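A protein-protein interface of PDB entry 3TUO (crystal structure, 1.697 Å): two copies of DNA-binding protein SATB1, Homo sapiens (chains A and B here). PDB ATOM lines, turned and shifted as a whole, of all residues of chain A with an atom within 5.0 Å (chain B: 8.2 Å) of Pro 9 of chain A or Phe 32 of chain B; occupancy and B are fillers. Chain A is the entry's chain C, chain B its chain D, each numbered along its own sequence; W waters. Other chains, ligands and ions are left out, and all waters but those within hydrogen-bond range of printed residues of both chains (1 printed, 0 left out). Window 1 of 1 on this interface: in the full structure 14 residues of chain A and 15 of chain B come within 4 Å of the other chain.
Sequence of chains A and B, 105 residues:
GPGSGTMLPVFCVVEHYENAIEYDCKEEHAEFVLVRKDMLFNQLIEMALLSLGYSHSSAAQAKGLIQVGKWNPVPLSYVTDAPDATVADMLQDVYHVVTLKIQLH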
ATOM      1  N   PRO A   2     -20.864 -13.040   1.217  1.00  0.00           N
ATOM      2  CA  PRO A   2     -22.049 -13.578   0.538  1.00  0.00           C
ATOM      3  C   PRO A   2     -21.722 -14.790  -0.328  1.00  0.00           C
ATOM      4  O   PRO A   2     -20.742 -14.774  -1.071  1.00  0.00           O
ATOM      5  CB  PRO A   2     -22.513 -12.405  -0.326  1.00  0.00           C
ATOM      6  CG  PRO A   2     -22.081 -11.197   0.440  1.00  0.00           C
ATOM      7  CD  PRO A   2     -20.760 -11.577   1.066  1.00  0.00           C
ATOM      8  N   GLY A   3     -22.539 -15.832  -0.216  1.00  0.00           N
ATOM      9  CA  GLY A   3     -22.333 -17.059  -0.960  1.00  0.00           C
ATOM     10  C   GLY A   3     -21.674 -18.141  -0.125  1.00  0.00           C
ATOM     11  O   GLY A   3     -21.539 -19.280  -0.571  1.00  0.00           O
ATOM     12  N   MET A   7     -26.879 -21.578  -0.237  1.00  0.00           N
ATOM     13  CA  MET A   7     -27.609 -21.193  -1.439  1.00  0.00           C
ATOM     14  C   MET A   7     -26.894 -20.088  -2.212  1.00  0.00           C
ATOM     15  O   MET A   7     -26.119 -19.318  -1.640  1.00  0.00           O
ATOM     16  CB  MET A   7     -29.011 -20.702  -1.067  1.00  0.00           C
ATOM     17  CG  MET A   7     -29.799 -21.650  -0.183  1.00  0.00           C
ATOM     18  SD  MET A   7     -30.226 -23.179  -1.038  1.00  0.00           S
ATOM     19  CE  MET A   7     -31.759 -22.714  -1.846  1.00  0.00           C
ATOM     20  N   LEU A   8     -27.164 -20.024  -3.513  1.00  0.00           N
ATOM     21  CA  LEU A   8     -26.822 -18.866  -4.329  1.00  0.00           C
ATOM     22  C   LEU A   8     -28.070 -18.374  -5.048  1.00  0.00           C
ATOM     23  O   LEU A   8     -28.878 -19.174  -5.526  1.00  0.00           O
ATOM     24  CB  LEU A   8     -25.753 -19.211  -5.370  1.00  0.00           C
ATOM     25  CG  LEU A   8     -24.325 -19.482  -4.899  1.00  0.00           C
ATOM     26  CD1 LEU A   8     -23.431 -19.794  -6.104  1.00  0.00           C
ATOM     27  CD2 LEU A   8     -23.776 -18.321  -4.075  1.00  0.00           C
ATOM     28  N   PRO A   9     -28.226 -17.055  -5.156  1.00  0.00           N
ATOM     29  CA  PRO A   9     -29.358 -16.509  -5.901  1.00  0.00           C
ATOM     30  C   PRO A   9     -29.045 -16.527  -7.388  1.00  0.00           C
ATOM     31  O   PRO A   9     -27.967 -16.082  -7.792  1.00  0.00           O
ATOM     32  CB  PRO A   9     -29.427 -15.055  -5.422  1.00  0.00           C
ATOM     33  CG  PRO A   9     -28.188 -14.825  -4.565  1.00  0.00           C
ATOM     34  CD  PRO A   9     -27.299 -16.006  -4.717  1.00  0.00           C
ATOM     35  N   VAL A  10     -29.960 -17.045  -8.195  1.00  0.00           N
ATOM     36  CA  VAL A  10     -29.799 -16.999  -9.641  1.00  0.00           C
ATOM     37  C   VAL A  10     -30.998 -16.285 -10.275  1.00  0.00           C
ATOM     38  O   VAL A  10     -32.140 -16.670 -10.049  1.00  0.00           O
ATOM     39  CB  VAL A  10     -29.664 -18.416 -10.230  1.00  0.00           C
ATOM     40  CG1 VAL A  10     -29.378 -18.348 -11.711  1.00  0.00           C
ATOM     41  CG2 VAL A  10     -28.559 -19.189  -9.514  1.00  0.00           C
ATOM     42  N   PHE A  11     -30.744 -15.238 -11.056  1.00  0.00           N
ATOM     43  CA  PHE A  11     -31.832 -14.516 -11.714  1.00  0.00           C
ATOM     44  C   PHE A  11     -32.320 -15.306 -12.926  1.00  0.00           C
ATOM     45  O   PHE A  11     -31.542 -15.624 -13.830  1.00  0.00           O
ATOM     46  CB  PHE A  11     -31.384 -13.117 -12.136  1.00  0.00           C
ATOM     47  CG  PHE A  11     -32.510 -12.226 -12.579  1.00  0.00           C
ATOM     48  CD1 PHE A  11     -33.449 -11.767 -11.667  1.00  0.00           C
ATOM     49  CD2 PHE A  11     -32.621 -11.831 -13.902  1.00  0.00           C
ATOM     50  CE1 PHE A  11     -34.481 -10.943 -12.071  1.00  0.00           C
ATOM     51  CE2 PHE A  11     -33.655 -11.008 -14.311  1.00  0.00           C
ATOM     52  CZ  PHE A  11     -34.586 -10.569 -13.397  1.00  0.00           C
ATOM     53  N   PHE A  32     -35.611 -13.817  -9.090  1.00  0.00           N
ATOM     54  CA  PHE A  32     -34.530 -14.550  -8.444  1.00  0.00           C
ATOM     55  C   PHE A  32     -35.027 -15.884  -7.880  1.00  0.00           C
ATOM     56  O   PHE A  32     -36.136 -15.976  -7.340  1.00  0.00           O
ATOM     57  CB  PHE A  32     -33.938 -13.737  -7.291  1.00  0.00           C
ATOM     58  CG  PHE A  32     -32.945 -12.700  -7.718  1.00  0.00           C
ATOM     59  CD1 PHE A  32     -31.659 -13.063  -8.101  1.00  0.00           C
ATOM     60  CD2 PHE A  32     -33.286 -11.355  -7.716  1.00  0.00           C
ATOM     61  CE1 PHE A  32     -30.728 -12.099  -8.479  1.00  0.00           C
ATOM     62  CE2 PHE A  32     -32.364 -10.389  -8.095  1.00  0.00           C
ATOM     63  CZ  PHE A  32     -31.083 -10.762  -8.481  1.00  0.00           C
ATOM     64  N   VAL A  33     -34.179 -16.901  -7.975  1.00  0.00           N
ATOM     65  CA  VAL A  33     -34.428 -18.187  -7.336  1.00  0.00           C
ATOM     66  C   VAL A  33     -33.215 -18.552  -6.489  1.00  0.00           C
ATOM     67  O   VAL A  33     -32.077 -18.276  -6.874  1.00  0.00           O
ATOM     68  CB  VAL A  33     -34.654 -19.293  -8.382  1.00  0.00           C
ATOM     69  CG1 VAL A  33     -34.684 -20.653  -7.715  1.00  0.00           C
ATOM     70  CG2 VAL A  33     -35.942 -19.041  -9.159  1.00  0.00           C
ATOM     71  N   LEU A  34     -33.445 -19.154  -5.329  1.00  0.00           N
ATOM     72  CA  LEU A  34     -32.333 -19.648  -4.535  1.00  0.00           C
ATOM     73  C   LEU A  34     -32.054 -21.108  -4.881  1.00  0.00           C
ATOM     74  O   LEU A  34     -32.953 -21.953  -4.836  1.00  0.00           O
ATOM     75  CB  LEU A  34     -32.604 -19.486  -3.039  1.00  0.00           C
ATOM     76  CG  LEU A  34     -32.789 -18.056  -2.526  1.00  0.00           C
ATOM     77  CD1 LEU A  34     -33.111 -18.063  -1.045  1.00  0.00           C
ATOM     78  CD2 LEU A  34     -31.556 -17.197  -2.806  1.00  0.00           C
ATOM     79  N   TYR A  95     -22.613 -14.949  -9.849  1.00  0.00           N
ATOM     80  CA  TYR A  95     -24.065 -15.039  -9.811  1.00  0.00           C
ATOM     81  C   TYR A  95     -24.759 -13.690  -9.999  1.00  0.00           C
ATOM     82  O   TYR A  95     -25.850 -13.628 -10.559  1.00  0.00           O
ATOM     83  CB  TYR A  95     -24.564 -15.743  -8.539  1.00  0.00           C
ATOM     84  CG  TYR A  95     -24.197 -15.047  -7.250  1.00  0.00           C
ATOM     85  CD1 TYR A  95     -25.023 -14.079  -6.703  1.00  0.00           C
ATOM     86  CD2 TYR A  95     -23.025 -15.364  -6.582  1.00  0.00           C
ATOM     87  CE1 TYR A  95     -24.682 -13.429  -5.516  1.00  0.00           C
ATOM     88  CE2 TYR A  95     -22.674 -14.727  -5.400  1.00  0.00           C
ATOM     89  CZ  TYR A  95     -23.511 -13.766  -4.871  1.00  0.00           C
ATOM     90  OH  TYR A  95     -23.160 -13.134  -3.696  1.00  0.00           O
ATOM     91  N   LEU B   8     -35.037  -9.045  -4.053  1.00  0.00           N
ATOM     92  CA  LEU B   8     -33.595  -8.868  -4.047  1.00  0.00           C
ATOM     93  C   LEU B   8     -33.003  -9.812  -3.016  1.00  0.00           C
ATOM     94  O   LEU B   8     -33.572  -9.992  -1.944  1.00  0.00           O
ATOM     95  CB  LEU B   8     -33.246  -7.427  -3.695  1.00  0.00           C
ATOM     96  CG  LEU B   8     -31.815  -7.006  -3.998  1.00  0.00           C
ATOM     97  CD1 LEU B   8     -31.592  -6.946  -5.506  1.00  0.00           C
ATOM     98  CD2 LEU B   8     -31.524  -5.664  -3.350  1.00  0.00           C
ATOM     99  N   PRO B   9     -31.868 -10.440  -3.338  1.00  0.00           N
ATOM    100  CA  PRO B   9     -31.249 -11.314  -2.338  1.00  0.00           C
ATOM    101  C   PRO B   9     -30.481 -10.487  -1.322  1.00  0.00           C
ATOM    102  O   PRO B   9     -29.791  -9.544  -1.699  1.00  0.00           O
ATOM    103  CB  PRO B   9     -30.265 -12.164  -3.162  1.00  0.00           C
ATOM    104  CG  PRO B   9     -30.607 -11.899  -4.610  1.00  0.00           C
ATOM    105  CD  PRO B   9     -31.196 -10.527  -4.644  1.00  0.00           C
ATOM    106  N   VAL B  10     -30.600 -10.830  -0.048  1.00  0.00           N
ATOM    107  CA  VAL B  10     -29.789 -10.198   0.985  1.00  0.00           C
ATOM    108  C   VAL B  10     -29.149 -11.284   1.835  1.00  0.00           C
ATOM    109  O   VAL B  10     -29.827 -12.203   2.302  1.00  0.00           O
ATOM    110  CB  VAL B  10     -30.615  -9.276   1.879  1.00  0.00           C
ATOM    111  CG1 VAL B  10     -29.692  -8.525   2.854  1.00  0.00           C
ATOM    112  CG2 VAL B  10     -31.417  -8.305   1.036  1.00  0.00           C
ATOM    113  N   PHE B  11     -27.838 -11.185   2.011  1.00  0.00           N
ATOM    114  CA  PHE B  11     -27.082 -12.161   2.780  1.00  0.00           C
ATOM    115  C   PHE B  11     -27.155 -11.736   4.241  1.00  0.00           C
ATOM    116  O   PHE B  11     -26.584 -10.712   4.613  1.00  0.00           O
ATOM    117  CB  PHE B  11     -25.637 -12.193   2.273  1.00  0.00           C
ATOM    118  CG  PHE B  11     -24.864 -13.415   2.691  1.00  0.00           C
ATOM    119  CD1 PHE B  11     -25.228 -14.675   2.238  1.00  0.00           C
ATOM    120  CD2 PHE B  11     -23.768 -13.300   3.529  1.00  0.00           C
ATOM    121  CE1 PHE B  11     -24.510 -15.802   2.620  1.00  0.00           C
ATOM    122  CE2 PHE B  11     -23.048 -14.420   3.911  1.00  0.00           C
ATOM    123  CZ  PHE B  11     -23.419 -15.672   3.455  1.00  0.00           C
ATOM    124  N   CYS B  12     -27.877 -12.520   5.046  1.00  0.00           N
ATOM    125  CA  CYS B  12     -28.276 -12.144   6.405  1.00  0.00           C
ATOM    126  C   CYS B  12     -27.870 -13.166   7.456  1.00  0.00           C
ATOM    127  O   CYS B  12     -27.778 -14.362   7.179  1.00  0.00           O
ATOM    128  CB  CYS B  12     -29.802 -12.009   6.482  1.00  0.00           C
ATOM    129  SG  CYS B  12     -30.501 -10.734   5.438  1.00  0.00           S
ATOM    130  N   VAL B  13     -27.669 -12.686   8.680  1.00  0.00           N
ATOM    131  CA  VAL B  13     -27.454 -13.558   9.820  1.00  0.00           C
ATOM    132  C   VAL B  13     -27.934 -12.864  11.082  1.00  0.00           C
ATOM    133  O   VAL B  13     -27.811 -11.641  11.215  1.00  0.00           O
ATOM    134  CB  VAL B  13     -25.969 -13.944   9.988  1.00  0.00           C
ATOM    135  CG1 VAL B  13     -25.138 -12.732  10.385  1.00  0.00           C
ATOM    136  CG2 VAL B  13     -25.831 -15.064  11.023  1.00  0.00           C
ATOM    137  N   HIS B  29     -25.583 -19.732  10.692  1.00  0.00           N
ATOM    138  CA  HIS B  29     -24.736 -19.325   9.577  1.00  0.00           C
ATOM    139  C   HIS B  29     -25.470 -18.352   8.661  1.00  0.00           C
ATOM    140  O   HIS B  29     -26.665 -18.499   8.412  1.00  0.00           O
ATOM    141  CB  HIS B  29     -24.267 -20.549   8.782  1.00  0.00           C
ATOM    142  CG  HIS B  29     -23.189 -20.250   7.787  1.00  0.00           C
ATOM    143  ND1 HIS B  29     -21.848 -20.350   8.089  1.00  0.00           N
ATOM    144  CD2 HIS B  29     -23.253 -19.852   6.493  1.00  0.00           C
ATOM    145  CE1 HIS B  29     -21.132 -20.027   7.026  1.00  0.00           C
ATOM    146  NE2 HIS B  29     -21.960 -19.719   6.044  1.00  0.00           N
ATOM    147  N   ALA B  30     -24.752 -17.351   8.169  1.00  0.00           N
ATOM    148  CA  ALA B  30     -25.339 -16.369   7.275  1.00  0.00           C
ATOM    149  C   ALA B  30     -25.895 -17.067   6.048  1.00  0.00           C
ATOM    150  O   ALA B  30     -25.311 -18.035   5.569  1.00  0.00           O
ATOM    151  CB  ALA B  30     -24.304 -15.335   6.872  1.00  0.00           C
ATOM    152  N   GLU B  31     -27.027 -16.576   5.552  1.00  0.00           N
ATOM    153  CA  GLU B  31     -27.654 -17.141   4.364  1.00  0.00           C
ATOM    154  C   GLU B  31     -28.395 -16.080   3.578  1.00  0.00           C
ATOM    155  O   GLU B  31     -28.795 -15.055   4.122  1.00  0.00           O
ATOM    156  CB  GLU B  31     -28.637 -18.253   4.737  1.00  0.00           C
ATOM    157  CG  GLU B  31     -28.010 -19.624   4.885  1.00  0.00           C
ATOM    158  CD  GLU B  31     -27.665 -20.279   3.553  1.00  0.00           C
ATOM    159  OE1 GLU B  31     -27.635 -19.594   2.503  1.00  0.00           O
ATOM    160  OE2 GLU B  31     -27.414 -21.495   3.567  1.00  0.00           O
ATOM    161  N   PHE B  32     -28.587 -16.343   2.293  1.00  0.00           N
ATOM    162  CA  PHE B  32     -29.374 -15.462   1.447  1.00  0.00           C
ATOM    163  C   PHE B  32     -30.858 -15.569   1.765  1.00  0.00           C
ATOM    164  O   PHE B  32     -31.387 -16.657   1.989  1.00  0.00           O
ATOM    165  CB  PHE B  32     -29.139 -15.775  -0.034  1.00  0.00           C
ATOM    166  CG  PHE B  32     -27.898 -15.148  -0.587  1.00  0.00           C
ATOM    167  CD1 PHE B  32     -27.827 -13.775  -0.770  1.00  0.00           C
ATOM    168  CD2 PHE B  32     -26.802 -15.929  -0.933  1.00  0.00           C
ATOM    169  CE1 PHE B  32     -26.676 -13.189  -1.284  1.00  0.00           C
ATOM    170  CE2 PHE B  32     -25.656 -15.350  -1.445  1.00  0.00           C
ATOM    171  CZ  PHE B  32     -25.594 -13.980  -1.622  1.00  0.00           C
ATOM    172  N   VAL B  33     -31.507 -14.414   1.781  1.00  0.00           N
ATOM    173  CA  VAL B  33     -32.944 -14.304   1.925  1.00  0.00           C
ATOM    174  C   VAL B  33     -33.440 -13.408   0.800  1.00  0.00           C
ATOM    175  O   VAL B  33     -32.763 -12.453   0.417  1.00  0.00           O
ATOM    176  CB  VAL B  33     -33.308 -13.646   3.264  1.00  0.00           C
ATOM    177  CG1 VAL B  33     -34.710 -13.059   3.201  1.00  0.00           C
ATOM    178  CG2 VAL B  33     -33.178 -14.647   4.397  1.00  0.00           C
ATOM    179  N   LEU B  34     -34.608 -13.720   0.252  1.00  0.00           N
ATOM    180  CA  LEU B  34     -35.200 -12.843  -0.745  1.00  0.00           C
ATOM    181  C   LEU B  34     -36.152 -11.883  -0.056  1.00  0.00           C
ATOM    182  O   LEU B  34     -36.993 -12.296   0.746  1.00  0.00           O
ATOM    183  CB  LEU B  34     -35.933 -13.642  -1.824  1.00  0.00           C
ATOM    184  CG  LEU B  34     -35.087 -14.561  -2.711  1.00  0.00           C
ATOM    185  CD1 LEU B  34     -35.977 -15.226  -3.742  1.00  0.00           C
ATOM    186  CD2 LEU B  34     -33.959 -13.798  -3.392  1.00  0.00           C
ATOM    187  N   VAL B  35     -36.009 -10.599  -0.353  1.00  0.00           N
ATOM    188  CA  VAL B  35     -36.896  -9.597   0.218  1.00  0.00           C
ATOM    189  C   VAL B  35     -37.401  -8.664  -0.875  1.00  0.00           C
ATOM    190  O   VAL B  35     -36.747  -8.498  -1.907  1.00  0.00           O
ATOM    191  CB  VAL B  35     -36.196  -8.788   1.323  1.00  0.00           C
ATOM    192  CG1 VAL B  35     -35.700  -9.713   2.422  1.00  0.00           C
ATOM    193  CG2 VAL B  35     -35.051  -7.990   0.745  1.00  0.00           C
ATOM    194  N   SER B  51     -38.215 -13.722   7.454  1.00  0.00           N
ATOM    195  CA  SER B  51     -37.776 -14.746   6.513  1.00  0.00           C
ATOM    196  C   SER B  51     -36.889 -15.800   7.168  1.00  0.00           C
ATOM    197  O   SER B  51     -36.785 -16.926   6.679  1.00  0.00           O
ATOM    198  CB  SER B  51     -37.046 -14.109   5.332  1.00  0.00           C
ATOM    199  OG  SER B  51     -37.934 -13.310   4.571  1.00  0.00           O
ATOM    200  N   LEU B  52     -36.254 -15.429   8.274  1.00  0.00           N
ATOM    201  CA  LEU B  52     -35.351 -16.333   8.981  1.00  0.00           C
ATOM    202  C   LEU B  52     -36.028 -17.083  10.125  1.00  0.00           C
ATOM    203  O   LEU B  52     -35.373 -17.857  10.824  1.00  0.00           O
ATOM    204  CB  LEU B  52     -34.138 -15.571   9.517  1.00  0.00           C
ATOM    205  CG  LEU B  52     -33.239 -14.926   8.462  1.00  0.00           C
ATOM    206  CD1 LEU B  52     -32.182 -14.069   9.123  1.00  0.00           C
ATOM    207  CD2 LEU B  52     -32.597 -15.993   7.583  1.00  0.00           C
ATOM    208  N   VAL B  94     -25.025  -3.760  -4.562  1.00  0.00           N
ATOM    209  CA  VAL B  94     -24.024  -4.263  -3.629  1.00  0.00           C
ATOM    210  C   VAL B  94     -24.400  -5.509  -2.838  1.00  0.00           C
ATOM    211  O   VAL B  94     -23.626  -5.953  -1.983  1.00  0.00           O
ATOM    212  CB  VAL B  94     -23.560  -3.172  -2.621  1.00  0.00           C
ATOM    213  CG1 VAL B  94     -23.018  -1.962  -3.358  1.00  0.00           C
ATOM    214  CG2 VAL B  94     -24.700  -2.774  -1.663  1.00  0.00           C
ATOM    215  N   TYR B  95     -25.563  -6.088  -3.114  1.00  0.00           N
ATOM    216  CA  TYR B  95     -26.014  -7.215  -2.303  1.00  0.00           C
ATOM    217  C   TYR B  95     -25.036  -8.399  -2.354  1.00  0.00           C
ATOM    218  O   TYR B  95     -25.053  -9.262  -1.479  1.00  0.00           O
ATOM    219  CB  TYR B  95     -27.428  -7.652  -2.702  1.00  0.00           C
ATOM    220  CG  TYR B  95     -27.493  -8.357  -4.028  1.00  0.00           C
ATOM    221  CD1 TYR B  95     -27.243  -9.717  -4.119  1.00  0.00           C
ATOM    222  CD2 TYR B  95     -27.819  -7.668  -5.187  1.00  0.00           C
ATOM    223  CE1 TYR B  95     -27.304 -10.375  -5.335  1.00  0.00           C
ATOM    224  CE2 TYR B  95     -27.888  -8.320  -6.410  1.00  0.00           C
ATOM    225  CZ  TYR B  95     -27.628  -9.672  -6.472  1.00  0.00           C
ATOM    226  OH  TYR B  95     -27.694 -10.324  -7.675  1.00  0.00           O
ATOM    227  N   HIS B  96     -24.177  -8.438  -3.369  1.00  0.00           N
ATOM    228  CA  HIS B  96     -23.231  -9.544  -3.494  1.00  0.00           C
ATOM    229  C   HIS B  96     -21.927  -9.326  -2.720  1.00  0.00           C
ATOM    230  O   HIS B  96     -21.071 -10.208  -2.702  1.00  0.00           O
ATOM    231  CB  HIS B  96     -22.916  -9.826  -4.968  1.00  0.00           C
ATOM    232  CG  HIS B  96     -22.269  -8.676  -5.672  1.00  0.00           C
ATOM    233  ND1 HIS B  96     -22.961  -7.538  -6.023  1.00  0.00           N
ATOM    234  CD2 HIS B  96     -20.993  -8.484  -6.080  1.00  0.00           C
ATOM    235  CE1 HIS B  96     -22.140  -6.692  -6.621  1.00  0.00           C
ATOM    236  NE2 HIS B  96     -20.939  -7.245  -6.669  1.00  0.00           N
ATOM    237  N   VAL B  97     -21.770  -8.169  -2.077  1.00  0.00           N
ATOM    238  CA  VAL B  97     -20.545  -7.926  -1.311  1.00  0.00           C
ATOM    239  C   VAL B  97     -20.804  -7.477   0.123  1.00  0.00           C
ATOM    240  O   VAL B  97     -19.866  -7.123   0.842  1.00  0.00           O
ATOM    241  CB  VAL B  97     -19.600  -6.877  -1.976  1.00  0.00           C
ATOM    242  CG1 VAL B  97     -19.084  -7.362  -3.329  1.00  0.00           C
ATOM    243  CG2 VAL B  97     -20.288  -5.523  -2.094  1.00  0.00           C
ATOM    244  N   VAL B  98     -22.064  -7.469   0.541  1.00  0.00           N
ATOM    245  CA  VAL B  98     -22.371  -7.035   1.901  1.00  0.00           C
ATOM    246  C   VAL B  98     -23.096  -8.113   2.683  1.00  0.00           C
ATOM    247  O   VAL B  98     -23.833  -8.913   2.115  1.00  0.00           O
ATOM    248  CB  VAL B  98     -23.181  -5.712   1.941  1.00  0.00           C
ATOM    249  CG1 VAL B  98     -22.492  -4.643   1.102  1.00  0.00           C
ATOM    250  CG2 VAL B  98     -24.605  -5.922   1.482  1.00  0.00           C
ATOM    251  N   THR B  99     -22.859  -8.133   3.991  1.00  0.00           N
ATOM    252  CA  THR B  99     -23.559  -9.042   4.886  1.00  0.00           C
ATOM    253  C   THR B  99     -24.295  -8.233   5.944  1.00  0.00           C
ATOM    254  O   THR B  99     -23.704  -7.366   6.595  1.00  0.00           O
ATOM    255  CB  THR B  99     -22.580 -10.003   5.593  1.00  0.00           C
ATOM    256  OG1 THR B  99     -21.838 -10.752   4.618  1.00  0.00           O
ATOM    257  CG2 THR B  99     -23.344 -10.971   6.512  1.00  0.00           C
HETATM  258  O   HOH W   1     -20.477 -12.682  -3.763  1.00  0.00           O
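N of Met 7 of chain A is in hydrogen-bond range of OE1 of Glu 31 of chain B, 3.5 Å away.
The backbone NH of Glu 31 of chain B is in hydrogen-bond range of the backbone carbonyl oxygen of Cys 12 of chain B (2.8 Å).
Among the printed residues, pairs that only touch across the chains: Tyr 95 of chain A with Phe 32 of chain B, Pro 2 of chain A with Val 98 of chain B, Gly 3 of chain A with Phe 32 of chain B, Pro 2 of chain A with His 96 of chain B, Gly 3 of chain A with Phe 11 of chain B, Pro 2 of chain A with Phe 11 of chain B, Pro 9 of chain A with Pro 9 of chain B, Phe 32 of chain A with Tyr 95 of chain B, Met 7 of chain A with Phe 32 of chain B, Tyr 95 of chain A with His 96 of chain B, Phe 32 of chain A with Pro 9 of chain B, Phe 32 of chain A with Leu 34 of chain B, Pro 2 of chain A with Phe 32 of chain B, Pro 9 of chain A with Phe 32 of chain B, Leu 34 of chain A with Phe 32 of chain B, Pro 2 of chain A with Thr 99 of chain B and Pro 2 of chain A with Val 97 of chain B.
Printed residues of chain B within 4 Å of Gly 3 of chain A: Phe 11 and Phe 32. Pro 9 of chain A touches just these residues of chain B: Pro 9 and Phe 32. Printed residues of chain B within 4 Å of Tyr 95 of chain A: Phe 32 and His 96. Val 10 of chain B touches none of the printed residues of chain A. Of chain A, only Pro 2, Gly 3, Met 7, Pro 9, Leu 34 and Tyr 95 come within 4 Å of Phe 32 of chain B. Val 33 of chain B touches none of the printed residues of chain A. The nearest printed residue of chain B that does not touch Pro 2 of chain A is Tyr 95 of chain B (4.03 Å).
Hydrophobic or aromatic side chains of chain B that line the printed part of chain A: Pro 9, Phe 11, Phe 32, Leu 34, Tyr 95 and His 96. Printed residues of chain A that touch a printed residue of chain B: Pro 2, Gly 3, Met 7, Pro 9, Phe 32, Leu 34 and Tyr 95. Hydrophobic or aromatic side chains of chain A within 4 Å of the printed part of chain B: Pro 2, Met 7, Pro 9, Phe 32, Leu 34 and Tyr 95.
Pro 9 of chain B touches its own counterpart, Pro 9 of chain A. Pro 9 of chain A touches Phe 32 of chain B, and with the chains exchanged Phe 32 of chain A touches Pro 9 of chain B. Phe 32 of chain A touches Leu 34 of chain B, and with the chains exchanged Leu 34 of chain A touches Phe 32 of chain B. Phe 32 of chain A touches Tyr 95 of chain B, and with the chains exchanged Tyr 95 of chain A touches Phe 32 of chain B. Positions printed for both chains: 8, 9, 10, 11, 32, 33, 34 and 95.
Water W1 lies within hydrogen-bond range of OH of Tyr 95 of chain A, O of His 96 of chain B and O of Pro 2 of chain A.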
